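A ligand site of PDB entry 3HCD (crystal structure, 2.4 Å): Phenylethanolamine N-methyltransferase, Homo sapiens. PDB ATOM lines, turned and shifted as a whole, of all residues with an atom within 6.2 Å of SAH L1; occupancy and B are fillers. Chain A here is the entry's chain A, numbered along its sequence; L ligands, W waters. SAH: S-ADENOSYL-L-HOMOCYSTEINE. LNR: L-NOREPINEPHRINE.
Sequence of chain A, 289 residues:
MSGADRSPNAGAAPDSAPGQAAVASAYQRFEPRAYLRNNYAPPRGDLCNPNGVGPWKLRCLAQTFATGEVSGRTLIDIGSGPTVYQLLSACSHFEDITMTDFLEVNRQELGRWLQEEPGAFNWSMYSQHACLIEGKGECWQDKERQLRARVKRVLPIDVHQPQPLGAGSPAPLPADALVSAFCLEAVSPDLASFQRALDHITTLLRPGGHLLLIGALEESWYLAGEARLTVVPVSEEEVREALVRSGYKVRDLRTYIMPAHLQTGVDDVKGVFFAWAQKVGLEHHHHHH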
ATOM      1  N   TYR A  27       0.785  25.102  26.283  1.00  0.00           N
ATOM      2  CA  TYR A  27      -0.584  25.293  25.811  1.00  0.00           C
ATOM      3  C   TYR A  27      -1.191  26.639  26.172  1.00  0.00           C
ATOM      4  O   TYR A  27      -2.243  27.024  25.632  1.00  0.00           O
ATOM      5  CB  TYR A  27      -1.507  24.137  26.247  1.00  0.00           C
ATOM      6  CG  TYR A  27      -1.452  22.980  25.262  1.00  0.00           C
ATOM      7  CD1 TYR A  27      -0.722  21.823  25.549  1.00  0.00           C
ATOM      8  CD2 TYR A  27      -2.089  23.060  24.026  1.00  0.00           C
ATOM      9  CE1 TYR A  27      -0.654  20.772  24.640  1.00  0.00           C
ATOM     10  CE2 TYR A  27      -2.023  22.022  23.110  1.00  0.00           C
ATOM     11  CZ  TYR A  27      -1.307  20.878  23.423  1.00  0.00           C
ATOM     12  OH  TYR A  27      -1.232  19.846  22.516  1.00  0.00           O
ATOM     13  N   PHE A  30      -1.253  28.671  23.127  1.00  0.00           N
ATOM     14  CA  PHE A  30      -1.998  28.070  22.010  1.00  0.00           C
ATOM     15  C   PHE A  30      -3.038  29.044  21.457  1.00  0.00           C
ATOM     16  O   PHE A  30      -3.918  29.495  22.181  1.00  0.00           O
ATOM     17  CB  PHE A  30      -2.699  26.813  22.507  1.00  0.00           C
ATOM     18  CG  PHE A  30      -3.464  26.067  21.448  1.00  0.00           C
ATOM     19  CD1 PHE A  30      -2.880  24.992  20.805  1.00  0.00           C
ATOM     20  CD2 PHE A  30      -4.772  26.406  21.144  1.00  0.00           C
ATOM     21  CE1 PHE A  30      -3.574  24.277  19.870  1.00  0.00           C
ATOM     22  CE2 PHE A  30      -5.476  25.705  20.208  1.00  0.00           C
ATOM     23  CZ  PHE A  30      -4.885  24.627  19.573  1.00  0.00           C
ATOM     24  N   TYR A  35      -4.207  27.698  14.845  1.00  0.00           N
ATOM     25  CA  TYR A  35      -4.311  26.259  14.731  1.00  0.00           C
ATOM     26  C   TYR A  35      -5.306  25.913  13.609  1.00  0.00           C
ATOM     27  O   TYR A  35      -4.963  25.151  12.693  1.00  0.00           O
ATOM     28  CB  TYR A  35      -4.750  25.651  16.050  1.00  0.00           C
ATOM     29  CG  TYR A  35      -4.977  24.155  15.983  1.00  0.00           C
ATOM     30  CD1 TYR A  35      -3.916  23.261  16.034  1.00  0.00           C
ATOM     31  CD2 TYR A  35      -6.279  23.631  15.886  1.00  0.00           C
ATOM     32  CE1 TYR A  35      -4.125  21.865  15.986  1.00  0.00           C
ATOM     33  CE2 TYR A  35      -6.501  22.248  15.851  1.00  0.00           C
ATOM     34  CZ  TYR A  35      -5.423  21.371  15.883  1.00  0.00           C
ATOM     35  OH  TYR A  35      -5.650  20.012  15.834  1.00  0.00           O
ATOM     36  N   TYR A  40      -6.971  23.508   8.982  1.00  0.00           N
ATOM     37  CA  TYR A  40      -8.329  23.422   8.490  1.00  0.00           C
ATOM     38  C   TYR A  40      -8.660  24.465   7.439  1.00  0.00           C
ATOM     39  O   TYR A  40      -9.804  24.574   7.058  1.00  0.00           O
ATOM     40  CB  TYR A  40      -9.314  23.422   9.660  1.00  0.00           C
ATOM     41  CG  TYR A  40      -9.023  22.243  10.581  1.00  0.00           C
ATOM     42  CD1 TYR A  40      -8.261  22.402  11.725  1.00  0.00           C
ATOM     43  CD2 TYR A  40      -9.455  20.973  10.251  1.00  0.00           C
ATOM     44  CE1 TYR A  40      -7.968  21.324  12.549  1.00  0.00           C
ATOM     45  CE2 TYR A  40      -9.172  19.901  11.045  1.00  0.00           C
ATOM     46  CZ  TYR A  40      -8.428  20.076  12.194  1.00  0.00           C
ATOM     47  OH  TYR A  40      -8.137  19.002  12.983  1.00  0.00           O
ATOM     48  N   LYS A  57     -10.320  11.669   6.845  1.00  0.00           N
ATOM     49  CA  LYS A  57     -10.858  11.653   8.194  1.00  0.00           C
ATOM     50  C   LYS A  57     -12.387  11.595   8.144  1.00  0.00           C
ATOM     51  O   LYS A  57     -13.006  10.803   8.857  1.00  0.00           O
ATOM     52  CB  LYS A  57     -10.354  12.889   8.961  1.00  0.00           C
ATOM     53  CG  LYS A  57      -8.879  12.822   9.408  1.00  0.00           C
ATOM     54  CD  LYS A  57      -8.441  14.044  10.244  1.00  0.00           C
ATOM     55  CE  LYS A  57      -8.679  15.343   9.475  1.00  0.00           C
ATOM     56  NZ  LYS A  57      -8.029  16.530  10.082  1.00  0.00           N
ATOM     57  N   ASP A  77     -16.960  14.300  23.339  1.00  0.00           N
ATOM     58  CA  ASP A  77     -15.833  14.591  22.465  1.00  0.00           C
ATOM     59  C   ASP A  77     -14.708  15.133  23.324  1.00  0.00           C
ATOM     60  O   ASP A  77     -14.802  16.240  23.860  1.00  0.00           O
ATOM     61  CB  ASP A  77     -16.206  15.609  21.373  1.00  0.00           C
ATOM     62  CG  ASP A  77     -15.066  15.851  20.371  1.00  0.00           C
ATOM     63  OD1 ASP A  77     -14.252  14.920  20.182  1.00  0.00           O
ATOM     64  OD2 ASP A  77     -14.999  16.951  19.751  1.00  0.00           O
ATOM     65  N   ILE A  78     -13.639  14.340  23.414  1.00  0.00           N
ATOM     66  CA  ILE A  78     -12.473  14.605  24.257  1.00  0.00           C
ATOM     67  C   ILE A  78     -11.436  15.476  23.557  1.00  0.00           C
ATOM     68  O   ILE A  78     -10.906  15.081  22.518  1.00  0.00           O
ATOM     69  CB  ILE A  78     -11.758  13.290  24.595  1.00  0.00           C
ATOM     70  CG1 ILE A  78     -12.726  12.315  25.236  1.00  0.00           C
ATOM     71  CG2 ILE A  78     -10.557  13.549  25.499  1.00  0.00           C
ATOM     72  CD1 ILE A  78     -13.387  12.891  26.442  1.00  0.00           C
ATOM     73  N   GLY A  79     -11.152  16.641  24.130  1.00  0.00           N
ATOM     74  CA  GLY A  79     -10.128  17.506  23.578  1.00  0.00           C
ATOM     75  C   GLY A  79     -10.527  18.075  22.221  1.00  0.00           C
ATOM     76  O   GLY A  79      -9.809  17.973  21.228  1.00  0.00           O
ATOM     77  N   SER A  80     -11.700  18.677  22.184  1.00  0.00           N
ATOM     78  CA  SER A  80     -12.293  19.165  20.957  1.00  0.00           C
ATOM     79  C   SER A  80     -11.473  20.293  20.357  1.00  0.00           C
ATOM     80  O   SER A  80     -11.457  20.520  19.138  1.00  0.00           O
ATOM     81  CB  SER A  80     -13.690  19.703  21.281  1.00  0.00           C
ATOM     82  OG  SER A  80     -14.534  18.668  21.723  1.00  0.00           O
ATOM     83  N   GLY A  81     -10.801  21.031  21.226  1.00  0.00           N
ATOM     84  CA  GLY A  81     -10.223  22.273  20.776  1.00  0.00           C
ATOM     85  C   GLY A  81     -11.254  23.168  20.101  1.00  0.00           C
ATOM     86  O   GLY A  81     -12.413  23.198  20.486  1.00  0.00           O
ATOM     87  N   PRO A  82     -10.816  23.895  19.077  1.00  0.00           N
ATOM     88  CA  PRO A  82     -11.710  24.799  18.357  1.00  0.00           C
ATOM     89  C   PRO A  82     -12.379  24.126  17.147  1.00  0.00           C
ATOM     90  O   PRO A  82     -12.665  24.860  16.209  1.00  0.00           O
ATOM     91  CB  PRO A  82     -10.751  25.875  17.830  1.00  0.00           C
ATOM     92  CG  PRO A  82      -9.343  25.270  17.962  1.00  0.00           C
ATOM     93  CD  PRO A  82      -9.465  23.898  18.511  1.00  0.00           C
ATOM     94  N   THR A  83     -12.595  22.813  17.143  1.00  0.00           N
ATOM     95  CA  THR A  83     -13.066  22.138  15.917  1.00  0.00           C
ATOM     96  C   THR A  83     -14.315  21.258  16.104  1.00  0.00           C
ATOM     97  O   THR A  83     -14.479  20.628  17.137  1.00  0.00           O
ATOM     98  CB  THR A  83     -11.965  21.280  15.247  1.00  0.00           C
ATOM     99  OG1 THR A  83     -11.734  20.081  15.988  1.00  0.00           O
ATOM    100  CG2 THR A  83     -10.672  22.058  15.084  1.00  0.00           C
ATOM    101  N   TYR A  85     -15.580  19.301  13.130  1.00  0.00           N
ATOM    102  CA  TYR A  85     -15.654  18.334  12.019  1.00  0.00           C
ATOM    103  C   TYR A  85     -15.727  16.895  12.523  1.00  0.00           C
ATOM    104  O   TYR A  85     -16.338  16.025  11.887  1.00  0.00           O
ATOM    105  CB  TYR A  85     -14.443  18.505  11.097  1.00  0.00           C
ATOM    106  CG  TYR A  85     -13.189  17.890  11.672  1.00  0.00           C
ATOM    107  CD1 TYR A  85     -12.867  16.560  11.409  1.00  0.00           C
ATOM    108  CD2 TYR A  85     -12.342  18.623  12.513  1.00  0.00           C
ATOM    109  CE1 TYR A  85     -11.716  15.971  11.964  1.00  0.00           C
ATOM    110  CE2 TYR A  85     -11.178  18.042  13.049  1.00  0.00           C
ATOM    111  CZ  TYR A  85     -10.893  16.714  12.789  1.00  0.00           C
ATOM    112  OH  TYR A  85      -9.748  16.139  13.315  1.00  0.00           O
ATOM    113  N   GLN A  86     -15.053  16.641  13.638  1.00  0.00           N
ATOM    114  CA  GLN A  86     -15.001  15.303  14.210  1.00  0.00           C
ATOM    115  C   GLN A  86     -16.374  14.807  14.662  1.00  0.00           C
ATOM    116  O   GLN A  86     -16.535  13.625  14.954  1.00  0.00           O
ATOM    117  CB  GLN A  86     -13.963  15.220  15.356  1.00  0.00           C
ATOM    118  CG  GLN A  86     -14.268  16.053  16.600  1.00  0.00           C
ATOM    119  CD  GLN A  86     -13.737  17.465  16.533  1.00  0.00           C
ATOM    120  OE1 GLN A  86     -13.519  18.016  15.448  1.00  0.00           O
ATOM    121  NE2 GLN A  86     -13.502  18.066  17.691  1.00  0.00           N
ATOM    122  N   THR A 100     -15.520  19.108  24.788  1.00  0.00           N
ATOM    123  CA  THR A 100     -14.624  19.438  25.875  1.00  0.00           C
ATOM    124  C   THR A 100     -13.291  19.981  25.391  1.00  0.00           C
ATOM    125  O   THR A 100     -12.840  19.682  24.287  1.00  0.00           O
ATOM    126  CB  THR A 100     -14.308  18.201  26.734  1.00  0.00           C
ATOM    127  OG1 THR A 100     -13.465  17.310  25.986  1.00  0.00           O
ATOM    128  CG2 THR A 100     -15.579  17.484  27.143  1.00  0.00           C
ATOM    129  N   ASP A 101     -12.657  20.775  26.242  1.00  0.00           N
ATOM    130  CA  ASP A 101     -11.267  21.122  26.025  1.00  0.00           C
ATOM    131  C   ASP A 101     -10.594  21.686  27.260  1.00  0.00           C
ATOM    132  O   ASP A 101     -11.262  22.103  28.190  1.00  0.00           O
ATOM    133  CB  ASP A 101     -11.123  22.115  24.892  1.00  0.00           C
ATOM    134  CG  ASP A 101      -9.711  22.157  24.370  1.00  0.00           C
ATOM    135  OD1 ASP A 101      -9.327  21.185  23.689  1.00  0.00           O
ATOM    136  OD2 ASP A 101      -9.014  23.150  24.649  1.00  0.00           O
ATOM    137  N   PHE A 102      -9.267  21.702  27.240  1.00  0.00           N
ATOM    138  CA  PHE A 102      -8.482  22.085  28.400  1.00  0.00           C
ATOM    139  C   PHE A 102      -8.435  23.605  28.530  1.00  0.00           C
ATOM    140  O   PHE A 102      -8.475  24.135  29.637  1.00  0.00           O
ATOM    141  CB  PHE A 102      -7.072  21.486  28.290  1.00  0.00           C
ATOM    142  CG  PHE A 102      -6.129  21.893  29.392  1.00  0.00           C
ATOM    143  CD1 PHE A 102      -6.190  21.288  30.639  1.00  0.00           C
ATOM    144  CD2 PHE A 102      -5.164  22.860  29.185  1.00  0.00           C
ATOM    145  CE1 PHE A 102      -5.320  21.651  31.667  1.00  0.00           C
ATOM    146  CE2 PHE A 102      -4.287  23.221  30.207  1.00  0.00           C
ATOM    147  CZ  PHE A 102      -4.374  22.625  31.450  1.00  0.00           C
ATOM    148  N   LEU A 103      -8.383  24.291  27.391  1.00  0.00           N
ATOM    149  CA  LEU A 103      -8.282  25.740  27.370  1.00  0.00           C
ATOM    150  C   LEU A 103      -9.639  26.429  27.304  1.00  0.00           C
ATOM    151  O   LEU A 103     -10.571  25.966  26.636  1.00  0.00           O
ATOM    152  CB  LEU A 103      -7.448  26.206  26.177  1.00  0.00           C
ATOM    153  CG  LEU A 103      -5.977  25.786  26.079  1.00  0.00           C
ATOM    154  CD1 LEU A 103      -5.396  26.232  24.746  1.00  0.00           C
ATOM    155  CD2 LEU A 103      -5.184  26.367  27.245  1.00  0.00           C
ATOM    156  N   ASN A 106     -10.424  27.889  23.672  1.00  0.00           N
ATOM    157  CA  ASN A 106     -11.003  26.969  22.689  1.00  0.00           C
ATOM    158  C   ASN A 106     -12.481  26.819  22.943  1.00  0.00           C
ATOM    159  O   ASN A 106     -13.267  26.897  22.009  1.00  0.00           O
ATOM    160  CB  ASN A 106     -10.311  25.610  22.709  1.00  0.00           C
ATOM    161  CG  ASN A 106      -8.989  25.624  21.976  1.00  0.00           C
ATOM    162  OD1 ASN A 106      -8.046  24.908  22.337  1.00  0.00           O
ATOM    163  ND2 ASN A 106      -8.909  26.433  20.908  1.00  0.00           N
ATOM    164  N   ILE A 157     -11.735  20.147  30.640  1.00  0.00           N
ATOM    165  CA  ILE A 157     -11.308  18.772  30.811  1.00  0.00           C
ATOM    166  C   ILE A 157      -9.790  18.726  30.899  1.00  0.00           C
ATOM    167  O   ILE A 157      -9.093  19.624  30.406  1.00  0.00           O
ATOM    168  CB  ILE A 157     -11.765  17.897  29.638  1.00  0.00           C
ATOM    169  CG1 ILE A 157     -11.590  16.417  29.973  1.00  0.00           C
ATOM    170  CG2 ILE A 157     -11.041  18.334  28.338  1.00  0.00           C
ATOM    171  CD1 ILE A 157     -12.051  15.466  28.855  1.00  0.00           C
ATOM    172  N   ASP A 158      -9.299  17.678  31.550  1.00  0.00           N
ATOM    173  CA  ASP A 158      -7.869  17.436  31.680  1.00  0.00           C
ATOM    174  C   ASP A 158      -7.684  15.934  31.680  1.00  0.00           C
ATOM    175  O   ASP A 158      -8.052  15.252  32.628  1.00  0.00           O
ATOM    176  CB  ASP A 158      -7.336  18.033  32.976  1.00  0.00           C
ATOM    177  CG  ASP A 158      -5.819  17.889  33.112  1.00  0.00           C
ATOM    178  OD1 ASP A 158      -5.232  16.980  32.495  1.00  0.00           O
ATOM    179  OD2 ASP A 158      -5.218  18.702  33.853  1.00  0.00           O
ATOM    180  N   VAL A 159      -7.129  15.397  30.590  1.00  0.00           N
ATOM    181  CA  VAL A 159      -7.025  13.941  30.460  1.00  0.00           C
ATOM    182  C   VAL A 159      -6.004  13.306  31.404  1.00  0.00           C
ATOM    183  O   VAL A 159      -5.967  12.086  31.564  1.00  0.00           O
ATOM    184  CB  VAL A 159      -6.713  13.512  29.006  1.00  0.00           C
ATOM    185  CG1 VAL A 159      -7.871  13.895  28.095  1.00  0.00           C
ATOM    186  CG2 VAL A 159      -5.380  14.128  28.546  1.00  0.00           C
ATOM    187  N   HIS A 160      -5.179  14.137  32.024  1.00  0.00           N
ATOM    188  CA  HIS A 160      -4.170  13.655  32.949  1.00  0.00           C
ATOM    189  C   HIS A 160      -4.777  13.292  34.302  1.00  0.00           C
ATOM    190  O   HIS A 160      -4.240  12.445  35.021  1.00  0.00           O
ATOM    191  CB  HIS A 160      -3.024  14.662  33.109  1.00  0.00           C
ATOM    192  CG  HIS A 160      -2.337  14.973  31.808  1.00  0.00           C
ATOM    193  ND1 HIS A 160      -1.780  14.003  31.014  1.00  0.00           N
ATOM    194  CD2 HIS A 160      -2.148  16.160  31.177  1.00  0.00           C
ATOM    195  CE1 HIS A 160      -1.263  14.569  29.932  1.00  0.00           C
ATOM    196  NE2 HIS A 160      -1.473  15.874  30.002  1.00  0.00           N
ATOM    197  N   SER A 180     -12.368  11.277  19.971  1.00  0.00           N
ATOM    198  CA  SER A 180     -11.249  12.155  20.288  1.00  0.00           C
ATOM    199  C   SER A 180     -10.297  12.230  19.116  1.00  0.00           C
ATOM    200  O   SER A 180      -9.904  11.203  18.577  1.00  0.00           O
ATOM    201  CB  SER A 180     -10.494  11.646  21.493  1.00  0.00           C
ATOM    202  OG  SER A 180      -9.415  12.508  21.783  1.00  0.00           O
ATOM    203  N   ALA A 181      -9.904  13.454  18.770  1.00  0.00           N
ATOM    204  CA  ALA A 181      -9.061  13.693  17.601  1.00  0.00           C
ATOM    205  C   ALA A 181      -7.851  14.551  17.922  1.00  0.00           C
ATOM    206  O   ALA A 181      -8.006  15.673  18.380  1.00  0.00           O
ATOM    207  CB  ALA A 181      -9.882  14.337  16.462  1.00  0.00           C
ATOM    208  N   PHE A 182      -6.650  14.021  17.680  1.00  0.00           N
ATOM    209  CA  PHE A 182      -5.405  14.769  17.888  1.00  0.00           C
ATOM    210  C   PHE A 182      -5.256  15.340  19.306  1.00  0.00           C
ATOM    211  O   PHE A 182      -4.689  16.413  19.513  1.00  0.00           O
ATOM    212  CB  PHE A 182      -5.289  15.912  16.862  1.00  0.00           C
ATOM    213  CG  PHE A 182      -5.378  15.447  15.448  1.00  0.00           C
ATOM    214  CD1 PHE A 182      -6.533  15.702  14.698  1.00  0.00           C
ATOM    215  CD2 PHE A 182      -4.364  14.697  14.876  1.00  0.00           C
ATOM    216  CE1 PHE A 182      -6.634  15.265  13.405  1.00  0.00           C
ATOM    217  CE2 PHE A 182      -4.466  14.260  13.582  1.00  0.00           C
ATOM    218  CZ  PHE A 182      -5.602  14.550  12.843  1.00  0.00           C
ATOM    219  N   CYS A 183      -5.769  14.599  20.290  1.00  0.00           N
ATOM    220  CA  CYS A 183      -5.703  15.032  21.672  1.00  0.00           C
ATOM    221  C   CYS A 183      -4.580  14.361  22.479  1.00  0.00           C
ATOM    222  O   CYS A 183      -3.579  14.992  22.817  1.00  0.00           O
ATOM    223  CB  CYS A 183      -7.035  14.781  22.363  1.00  0.00           C
ATOM    224  SG  CYS A 183      -6.949  15.427  24.081  1.00  0.00           S
ATOM    225  N   ALA A 186      -0.924  14.623  21.676  1.00  0.00           N
ATOM    226  CA  ALA A 186      -0.493  16.011  21.674  1.00  0.00           C
ATOM    227  C   ALA A 186      -0.396  16.601  23.071  1.00  0.00           C
ATOM    228  O   ALA A 186       0.158  17.683  23.227  1.00  0.00           O
ATOM    229  CB  ALA A 186      -1.441  16.860  20.809  1.00  0.00           C
ATOM    230  N   VAL A 187      -0.936  15.921  24.082  1.00  0.00           N
ATOM    231  CA  VAL A 187      -0.846  16.441  25.462  1.00  0.00           C
ATOM    232  C   VAL A 187       0.041  15.588  26.383  1.00  0.00           C
ATOM    233  O   VAL A 187       0.236  15.906  27.557  1.00  0.00           O
ATOM    234  CB  VAL A 187      -2.231  16.612  26.121  1.00  0.00           C
ATOM    235  CG1 VAL A 187      -3.087  17.543  25.291  1.00  0.00           C
ATOM    236  CG2 VAL A 187      -2.908  15.274  26.306  1.00  0.00           C
ATOM    237  N   ILE A 214      -8.878   9.485  16.485  1.00  0.00           N
ATOM    238  CA  ILE A 214      -8.085   9.960  15.351  1.00  0.00           C
ATOM    239  C   ILE A 214      -6.845  10.630  15.936  1.00  0.00           C
ATOM    240  O   ILE A 214      -6.944  11.269  16.980  1.00  0.00           O
ATOM    241  CB  ILE A 214      -8.879  10.977  14.504  1.00  0.00           C
ATOM    242  CG1 ILE A 214     -10.056  10.282  13.813  1.00  0.00           C
ATOM    243  CG2 ILE A 214      -8.013  11.645  13.442  1.00  0.00           C
ATOM    244  CD1 ILE A 214     -11.153  11.283  13.310  1.00  0.00           C
ATOM    245  N   TYR A 222       3.974  20.576  16.655  1.00  0.00           N
ATOM    246  CA  TYR A 222       3.150  21.354  15.740  1.00  0.00           C
ATOM    247  C   TYR A 222       2.974  22.751  16.301  1.00  0.00           C
ATOM    248  O   TYR A 222       3.094  22.976  17.514  1.00  0.00           O
ATOM    249  CB  TYR A 222       1.795  20.680  15.469  1.00  0.00           C
ATOM    250  CG  TYR A 222       0.838  20.735  16.623  1.00  0.00           C
ATOM    251  CD1 TYR A 222      -0.151  21.703  16.683  1.00  0.00           C
ATOM    252  CD2 TYR A 222       0.911  19.813  17.657  1.00  0.00           C
ATOM    253  CE1 TYR A 222      -1.033  21.770  17.747  1.00  0.00           C
ATOM    254  CE2 TYR A 222       0.031  19.868  18.743  1.00  0.00           C
ATOM    255  CZ  TYR A 222      -0.928  20.848  18.772  1.00  0.00           C
ATOM    256  OH  TYR A 222      -1.816  20.909  19.813  1.00  0.00           O
HETATM  257  N   SAH L   1      -9.738  17.766  18.357  1.00  0.00           N
HETATM  258  CA  SAH L   1      -9.423  18.815  17.412  1.00  0.00           C
HETATM  259  CB  SAH L   1      -8.436  19.803  18.014  1.00  0.00           C
HETATM  260  CG  SAH L   1      -7.253  19.050  18.648  1.00  0.00           C
HETATM  261  SD  SAH L   1      -5.836  20.052  19.235  1.00  0.00           S
HETATM  262  C   SAH L   1      -8.838  18.293  16.112  1.00  0.00           C
HETATM  263  O   SAH L   1      -9.425  17.155  15.565  1.00  0.00           O
HETATM  264  OXT SAH L   1      -8.263  19.103  15.501  1.00  0.00           O
HETATM  265  C5' SAH L   1      -5.510  19.381  20.894  1.00  0.00           C
HETATM  266  C4' SAH L   1      -6.445  19.998  21.929  1.00  0.00           C
HETATM  267  O4' SAH L   1      -5.976  19.409  23.088  1.00  0.00           O
HETATM  268  C3' SAH L   1      -6.327  21.519  22.161  1.00  0.00           C
HETATM  269  O3' SAH L   1      -7.587  22.150  21.992  1.00  0.00           O
HETATM  270  C2' SAH L   1      -5.886  21.553  23.474  1.00  0.00           C
HETATM  271  O2' SAH L   1      -6.234  22.665  24.263  1.00  0.00           O
HETATM  272  C1' SAH L   1      -6.318  20.338  24.044  1.00  0.00           C
HETATM  273  N9  SAH L   1      -5.705  20.009  25.320  1.00  0.00           N
HETATM  274  C8  SAH L   1      -4.551  20.483  25.803  1.00  0.00           C
HETATM  275  N7  SAH L   1      -4.296  19.858  27.004  1.00  0.00           N
HETATM  276  C5  SAH L   1      -5.311  18.979  27.250  1.00  0.00           C
HETATM  277  C6  SAH L   1      -5.589  18.124  28.270  1.00  0.00           C
HETATM  278  N6  SAH L   1      -4.635  18.054  29.340  1.00  0.00           N
HETATM  279  N1  SAH L   1      -6.680  17.361  28.301  1.00  0.00           N
HETATM  280  C2  SAH L   1      -7.550  17.452  27.278  1.00  0.00           C
HETATM  281  N3  SAH L   1      -7.287  18.311  26.271  1.00  0.00           N
HETATM  282  C4  SAH L   1      -6.182  19.070  26.241  1.00  0.00           C
HETATM  283  OAC LNR L   2      -5.928  18.173  11.651  1.00  0.00           O
HETATM  284  CAJ LNR L   2      -4.559  17.887  11.657  1.00  0.00           C
HETATM  285  CAG LNR L   2      -3.774  17.985  12.803  1.00  0.00           C
HETATM  286  CAI LNR L   2      -3.978  17.454  10.466  1.00  0.00           C
HETATM  287  OAB LNR L   2      -4.720  17.428   9.299  1.00  0.00           O
HETATM  288  CAE LNR L   2      -2.638  17.120  10.389  1.00  0.00           C
HETATM  289  CAF LNR L   2      -1.853  17.218  11.535  1.00  0.00           C
HETATM  290  CAK LNR L   2      -2.404  17.651  12.730  1.00  0.00           C
HETATM  291  CAL LNR L   2      -1.500  17.692  13.975  1.00  0.00           C
HETATM  292  OAD LNR L   2      -0.691  18.829  14.051  1.00  0.00           O
HETATM  293  CAH LNR L   2      -2.356  17.557  15.237  1.00  0.00           C
HETATM  294  NAA LNR L   2      -1.603  18.015  16.380  1.00  0.00           N
HETATM  295  O   HOH W   1     -11.500  15.889  19.729  1.00  0.00           O
HETATM  296  O   HOH W   2      -1.768  19.212  30.476  1.00  0.00           O
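The side-chain sulfur of Cys 183 lies within hydrogen-bond range of a nitrogen (N3) of SAH L1 (3.6 Å). The side-chain hydroxyl (OH) of Tyr 35 is in hydrogen-bond range of an oxygen (OXT) of SAH L1 (2.8 Å). OD1 of Asp 158 sits at hydrogen-bond distance from N6 of SAH L1 (3.4 Å). NZ of Lys 57 is in hydrogen-bond range of OAC of LNR L2, 3.1 Å away. The backbone carbonyl oxygen of Ser 80 lies close to a nitrogen (N) of SAH L1 (3.3 Å). The backbone NH of Gly 81 lies close to an oxygen (O3') of SAH L1 (3.5 Å). OH of Tyr 40 lies within hydrogen-bond range of OAC of LNR L2 (2.7 Å). N of Val 159 sits at hydrogen-bond distance from N1 of SAH L1. A nitrogen (N) of SAH L1 lies within hydrogen-bond range of the backbone carbonyl oxygen (O) of Gly 79, at 2.9 Å. N of SAH L1 sits at hydrogen-bond distance from O of Ala 181 (2.7 Å). OD1 of Asp 101 sits at hydrogen-bond distance from O3' of SAH L1, at 2.6 Å. The side-chain amide oxygen (OD1) of Asn 106 is in hydrogen-bond range of an oxygen (O3') of SAH L1 (2.8 Å). O of SAH L1 lies within hydrogen-bond range of OH of Tyr 85. OXT of SAH L1 is in hydrogen-bond range of OH of Tyr 40 (2.5 Å).
The side-chain amide oxygen (OD1) of Asn 106 lies close to the side-chain carboxylate (OD2) of Asp 101, at 3.1 Å. The backbone NH (N) of Ser 80 sits at hydrogen-bond distance from the backbone carbonyl oxygen (O) of Thr 100 (2.6 Å). The backbone NH (N) of Gly 79 lies within hydrogen-bond range of the side-chain hydroxyl (OG1) of Thr 100 (3.0 Å). OD1 of Asp 158 lies within hydrogen-bond range of N of His 160, 2.9 Å away. The side-chain carboxylate (OD2) of Asp 77 sits at hydrogen-bond distance from the side-chain amide nitrogen (NE2) of Gln 86 (2.8 Å). The backbone carbonyl oxygen (O) of Val 187 is in hydrogen-bond range of a ring nitrogen (NE2) of His 160 (3.0 Å). The backbone NH (N) of Gly 81 is in hydrogen-bond range of the side-chain carboxylate (OD1) of Asp 101 (2.9 Å). The side-chain hydroxyl of Thr 83 lies within hydrogen-bond range of the side-chain amide oxygen of Gln 86 (2.8 Å).
Merely in contact with SAH L1: Tyr 27, Thr 83, Gln 86, Phe 102, Leu 103, Ile 157, His 160, Phe 182 and Val 187. Hydrophobic or aromatic side chains that line SAH L1: Tyr 27, Tyr 35, Tyr 40, Tyr 85, Phe 102, Leu 103, Ile 157, Val 159, His 160, Ala 181, Phe 182 and Val 187. Of the 31 residues printed, 21 come within 4 Å of SAH L1.
Water W2 lies within hydrogen-bond range of a nitrogen (N6) of SAH L1 and a ring nitrogen (NE2) of His 160.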
